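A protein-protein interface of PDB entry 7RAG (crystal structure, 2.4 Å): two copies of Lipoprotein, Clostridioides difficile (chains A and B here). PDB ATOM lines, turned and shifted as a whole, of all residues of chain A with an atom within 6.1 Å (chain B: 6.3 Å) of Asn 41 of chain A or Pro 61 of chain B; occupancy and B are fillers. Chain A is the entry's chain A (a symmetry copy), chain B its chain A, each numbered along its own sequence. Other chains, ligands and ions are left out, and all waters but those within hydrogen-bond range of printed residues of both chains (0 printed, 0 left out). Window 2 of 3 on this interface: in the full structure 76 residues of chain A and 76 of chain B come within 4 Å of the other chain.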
ATOM      1  N   VAL A  31       2.878 -16.337  27.284  1.00  0.00           N
ATOM      2  CA  VAL A  31       3.153 -17.624  27.904  1.00  0.00           C
ATOM      3  C   VAL A  31       3.137 -17.455  29.411  1.00  0.00           C
ATOM      4  O   VAL A  31       3.835 -16.591  29.949  1.00  0.00           O
ATOM      5  CB  VAL A  31       4.503 -18.198  27.447  1.00  0.00           C
ATOM      6  CG1 VAL A  31       4.706 -19.556  28.061  1.00  0.00           C
ATOM      7  CG2 VAL A  31       4.577 -18.258  25.926  1.00  0.00           C
ATOM      8  N   GLU A  32       2.351 -18.280  30.093  1.00  0.00           N
ATOM      9  CA  GLU A  32       2.401 -18.402  31.546  1.00  0.00           C
ATOM     10  C   GLU A  32       3.115 -19.704  31.916  1.00  0.00           C
ATOM     11  O   GLU A  32       2.768 -20.782  31.411  1.00  0.00           O
ATOM     12  CB  GLU A  32       0.993 -18.370  32.143  1.00  0.00           C
ATOM     13  CG  GLU A  32       1.006 -18.367  33.666  1.00  0.00           C
ATOM     14  CD  GLU A  32      -0.353 -18.700  34.322  1.00  0.00           C
ATOM     15  OE1 GLU A  32      -0.891 -19.817  34.092  1.00  0.00           O
ATOM     16  OE2 GLU A  32      -0.864 -17.856  35.094  1.00  0.00           O
ATOM     17  N   VAL A  33       4.123 -19.601  32.773  1.00  0.00           N
ATOM     18  CA  VAL A  33       4.890 -20.752  33.237  1.00  0.00           C
ATOM     19  C   VAL A  33       4.690 -20.866  34.731  1.00  0.00           C
ATOM     20  O   VAL A  33       4.818 -19.871  35.453  1.00  0.00           O
ATOM     21  CB  VAL A  33       6.384 -20.626  32.891  1.00  0.00           C
ATOM     22  CG1 VAL A  33       7.140 -21.890  33.310  1.00  0.00           C
ATOM     23  CG2 VAL A  33       6.558 -20.350  31.381  1.00  0.00           C
ATOM     24  N   PRO A  39       3.557 -18.168  39.334  1.00  0.00           N
ATOM     25  CA  PRO A  39       3.708 -18.183  37.880  1.00  0.00           C
ATOM     26  C   PRO A  39       4.524 -16.982  37.418  1.00  0.00           C
ATOM     27  O   PRO A  39       4.749 -16.022  38.159  1.00  0.00           O
ATOM     28  CB  PRO A  39       2.266 -18.122  37.357  1.00  0.00           C
ATOM     29  CG  PRO A  39       1.451 -17.661  38.485  1.00  0.00           C
ATOM     30  CD  PRO A  39       2.149 -18.062  39.751  1.00  0.00           C
ATOM     31  N   HIS A  40       5.043 -17.091  36.199  1.00  0.00           N
ATOM     32  CA  HIS A  40       5.789 -16.025  35.552  1.00  0.00           C
ATOM     33  C   HIS A  40       5.252 -15.884  34.137  1.00  0.00           C
ATOM     34  O   HIS A  40       4.815 -16.866  33.526  1.00  0.00           O
ATOM     35  CB  HIS A  40       7.291 -16.331  35.527  1.00  0.00           C
ATOM     36  CG  HIS A  40       8.161 -15.120  35.637  1.00  0.00           C
ATOM     37  ND1 HIS A  40       8.456 -14.525  36.847  1.00  0.00           N
ATOM     38  CD2 HIS A  40       8.806 -14.392  34.697  1.00  0.00           C
ATOM     39  CE1 HIS A  40       9.244 -13.483  36.645  1.00  0.00           C
ATOM     40  NE2 HIS A  40       9.475 -13.380  35.348  1.00  0.00           N
ATOM     41  N   ASN A  41       5.272 -14.671  33.613  1.00  0.00           N
ATOM     42  CA  ASN A  41       4.693 -14.445  32.300  1.00  0.00           C
ATOM     43  C   ASN A  41       5.753 -13.940  31.330  1.00  0.00           C
ATOM     44  O   ASN A  41       6.750 -13.336  31.725  1.00  0.00           O
ATOM     45  CB  ASN A  41       3.501 -13.521  32.400  1.00  0.00           C
ATOM     46  CG  ASN A  41       2.331 -14.187  33.138  1.00  0.00           C
ATOM     47  OD1 ASN A  41       1.797 -15.188  32.677  1.00  0.00           O
ATOM     48  ND2 ASN A  41       1.971 -13.667  34.296  1.00  0.00           N
ATOM     49  N   TYR A  42       5.598 -14.319  30.066  1.00  0.00           N
ATOM     50  CA  TYR A  42       6.522 -13.929  29.026  1.00  0.00           C
ATOM     51  C   TYR A  42       5.712 -13.555  27.801  1.00  0.00           C
ATOM     52  O   TYR A  42       4.605 -14.060  27.616  1.00  0.00           O
ATOM     53  CB  TYR A  42       7.483 -15.061  28.687  1.00  0.00           C
ATOM     54  CG  TYR A  42       8.199 -15.599  29.882  1.00  0.00           C
ATOM     55  CD1 TYR A  42       9.440 -15.100  30.248  1.00  0.00           C
ATOM     56  CD2 TYR A  42       7.644 -16.623  30.638  1.00  0.00           C
ATOM     57  CE1 TYR A  42      10.105 -15.592  31.343  1.00  0.00           C
ATOM     58  CE2 TYR A  42       8.301 -17.126  31.725  1.00  0.00           C
ATOM     59  CZ  TYR A  42       9.532 -16.602  32.081  1.00  0.00           C
ATOM     60  OH  TYR A  42      10.184 -17.112  33.183  1.00  0.00           O
ATOM     61  N   VAL A  43       6.252 -12.671  26.967  1.00  0.00           N
ATOM     62  CA  VAL A  43       5.676 -12.449  25.650  1.00  0.00           C
ATOM     63  C   VAL A  43       6.760 -12.661  24.610  1.00  0.00           C
ATOM     64  O   VAL A  43       7.844 -12.073  24.687  1.00  0.00           O
ATOM     65  CB  VAL A  43       5.026 -11.063  25.505  1.00  0.00           C
ATOM     66  CG1 VAL A  43       4.534 -10.858  24.105  1.00  0.00           C
ATOM     67  CG2 VAL A  43       3.854 -10.942  26.454  1.00  0.00           C
ATOM     68  N   VAL B  58      11.955 -12.925  22.304  1.00  0.00           N
ATOM     69  CA  VAL B  58      11.295 -12.458  23.512  1.00  0.00           C
ATOM     70  C   VAL B  58      11.221 -10.941  23.498  1.00  0.00           C
ATOM     71  O   VAL B  58      12.215 -10.258  23.220  1.00  0.00           O
ATOM     72  CB  VAL B  58      12.024 -12.947  24.767  1.00  0.00           C
ATOM     73  CG1 VAL B  58      11.131 -12.706  25.945  1.00  0.00           C
ATOM     74  CG2 VAL B  58      12.369 -14.410  24.644  1.00  0.00           C
ATOM     75  N   ILE B  59      10.042 -10.407  23.818  1.00  0.00           N
ATOM     76  CA  ILE B  59       9.840  -8.971  23.878  1.00  0.00           C
ATOM     77  C   ILE B  59       9.498  -8.493  25.283  1.00  0.00           C
ATOM     78  O   ILE B  59      10.002  -7.454  25.715  1.00  0.00           O
ATOM     79  CB  ILE B  59       8.772  -8.500  22.866  1.00  0.00           C
ATOM     80  CG1 ILE B  59       7.446  -9.209  23.060  1.00  0.00           C
ATOM     81  CG2 ILE B  59       9.249  -8.695  21.432  1.00  0.00           C
ATOM     82  CD1 ILE B  59       6.353  -8.633  22.178  1.00  0.00           C
ATOM     83  N   SER B  60       8.635  -9.225  26.020  1.00  0.00           N
ATOM     84  CA  SER B  60       8.011  -8.539  27.156  1.00  0.00           C
ATOM     85  C   SER B  60       8.885  -8.376  28.389  1.00  0.00           C
ATOM     86  O   SER B  60       9.129  -7.226  28.791  1.00  0.00           O
ATOM     87  CB  SER B  60       6.724  -9.198  27.628  1.00  0.00           C
ATOM     88  OG  SER B  60       6.558  -8.937  29.010  1.00  0.00           O
ATOM     89  N   PRO B  61       9.329  -9.443  29.062  1.00  0.00           N
ATOM     90  CA  PRO B  61      10.097  -9.201  30.297  1.00  0.00           C
ATOM     91  C   PRO B  61      11.379  -8.509  29.871  1.00  0.00           C
ATOM     92  O   PRO B  61      12.143  -9.040  29.066  1.00  0.00           O
ATOM     93  CB  PRO B  61      10.325 -10.604  30.889  1.00  0.00           C
ATOM     94  CG  PRO B  61       9.516 -11.542  30.029  1.00  0.00           C
ATOM     95  CD  PRO B  61       9.307 -10.869  28.690  1.00  0.00           C
ATOM     96  N   LYS B  62      11.576  -7.284  30.363  1.00  0.00           N
ATOM     97  CA  LYS B  62      12.603  -6.402  29.802  1.00  0.00           C
ATOM     98  C   LYS B  62      13.970  -7.076  29.750  1.00  0.00           C
ATOM     99  O   LYS B  62      14.724  -6.908  28.780  1.00  0.00           O
ATOM    100  CB  LYS B  62      12.691  -5.115  30.620  1.00  0.00           C
ATOM    101  CG  LYS B  62      13.401  -4.006  29.896  1.00  0.00           C
ATOM    102  CD  LYS B  62      14.680  -3.623  30.578  1.00  0.00           C
ATOM    103  CE  LYS B  62      15.019  -2.175  30.259  1.00  0.00           C
ATOM    104  NZ  LYS B  62      13.944  -1.229  30.731  1.00  0.00           N
ATOM    105  N   HIS B  63      14.292  -7.863  30.781  1.00  0.00           N
ATOM    106  CA  HIS B  63      15.565  -8.575  30.830  1.00  0.00           C
ATOM    107  C   HIS B  63      15.782  -9.411  29.572  1.00  0.00           C
ATOM    108  O   HIS B  63      16.915  -9.537  29.088  1.00  0.00           O
ATOM    109  CB  HIS B  63      15.605  -9.449  32.094  1.00  0.00           C
ATOM    110  CG  HIS B  63      16.647 -10.524  32.067  1.00  0.00           C
ATOM    111  ND1 HIS B  63      16.427 -11.781  32.587  1.00  0.00           N
ATOM    112  CD2 HIS B  63      17.908 -10.537  31.575  1.00  0.00           C
ATOM    113  CE1 HIS B  63      17.506 -12.521  32.412  1.00  0.00           C
ATOM    114  NE2 HIS B  63      18.421 -11.788  31.806  1.00  0.00           N
ATOM    115  N   LEU B  64      14.712  -9.992  29.031  1.00  0.00           N
ATOM    116  CA  LEU B  64      14.843 -10.912  27.910  1.00  0.00           C
ATOM    117  C   LEU B  64      14.646 -10.255  26.555  1.00  0.00           C
ATOM    118  O   LEU B  64      14.927 -10.894  25.536  1.00  0.00           O
ATOM    119  CB  LEU B  64      13.845 -12.054  28.053  1.00  0.00           C
ATOM    120  CG  LEU B  64      13.983 -12.891  29.318  1.00  0.00           C
ATOM    121  CD1 LEU B  64      12.941 -13.987  29.316  1.00  0.00           C
ATOM    122  CD2 LEU B  64      15.360 -13.464  29.473  1.00  0.00           C
ATOM    123  N   LYS B  65      14.186  -9.006  26.526  1.00  0.00           N
ATOM    124  CA  LYS B  65      13.797  -8.352  25.285  1.00  0.00           C
ATOM    125  C   LYS B  65      14.913  -8.451  24.260  1.00  0.00           C
ATOM    126  O   LYS B  65      16.073  -8.168  24.562  1.00  0.00           O
ATOM    127  CB  LYS B  65      13.461  -6.888  25.563  1.00  0.00           C
ATOM    128  CG  LYS B  65      13.033  -6.078  24.353  1.00  0.00           C
ATOM    129  CD  LYS B  65      13.006  -4.575  24.679  1.00  0.00           C
ATOM    130  CE  LYS B  65      12.432  -3.766  23.536  1.00  0.00           C
ATOM    131  NZ  LYS B  65      12.628  -2.277  23.680  1.00  0.00           N
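Printed residues of chain A that touch a printed residue of chain B: Asn 41, Tyr 42 and Val 43.
Hydrophobic or aromatic side chains of chain A that line the printed part of chain B: Tyr 42 and Val 43.
Along chain A the printed residues that touch a printed residue of chain B span positions 41 to 43.
Asn 41 of chain A touches Pro 61 of chain B.
Pro 61 of chain B touches Tyr 42 of chain A (CG to CD1, 3.6 Å).
CD1 of Leu 64 of chain B touches CD1 of Tyr 42 of chain A (3.8 Å).
Val 58 of chain B touches Val 43 of chain A (CG1 to O, 3.6 Å).
CD of Pro 61 of chain B touches N of Val 43 of chain A, at 3.9 Å.
No position is printed for both chains.
Asn 41 of chain A touches just one residue of chain B: Pro 61.
Of chain A, only Asn 41, Tyr 42 and Val 43 come within 4 Å of Pro 61 of chain B.
Printed residues of chain A within 4 Å of Leu 64 of chain B: Tyr 42.
Of the printed residues of chain B, Tyr 42 of chain A touches Pro 61 (3.6 Å) and Leu 64 (3.8 Å).
Printed residues of chain B within 4 Å of Val 43 of chain A: Val 58, Ile 59, Ser 60 and Pro 61.
Of the printed residues of chain A, Ser 60 of chain B touches Val 43 (3.2 Å).
Glu 32 of chain A touches none of the printed residues of chain B.
Pro 39 of chain A touches none of the printed residues of chain B.
The nearest printed residue of chain A that does not touch Ser 60 of chain B is Tyr 42 of chain A (4.5 Å).
The backbone carbonyl oxygen (O) of Val 43 of chain A lies within hydrogen-bond range of the backbone NH (N) of Ile 59 of chain B, at 2.9 Å.
N of Ser 60 of chain B lies within hydrogen-bond range of O of Val 43 of chain A (3.2 Å).
O of Tyr 42 of chain A is in hydrogen-bond range of N of Val 31 of chain A, at 2.9 Å.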
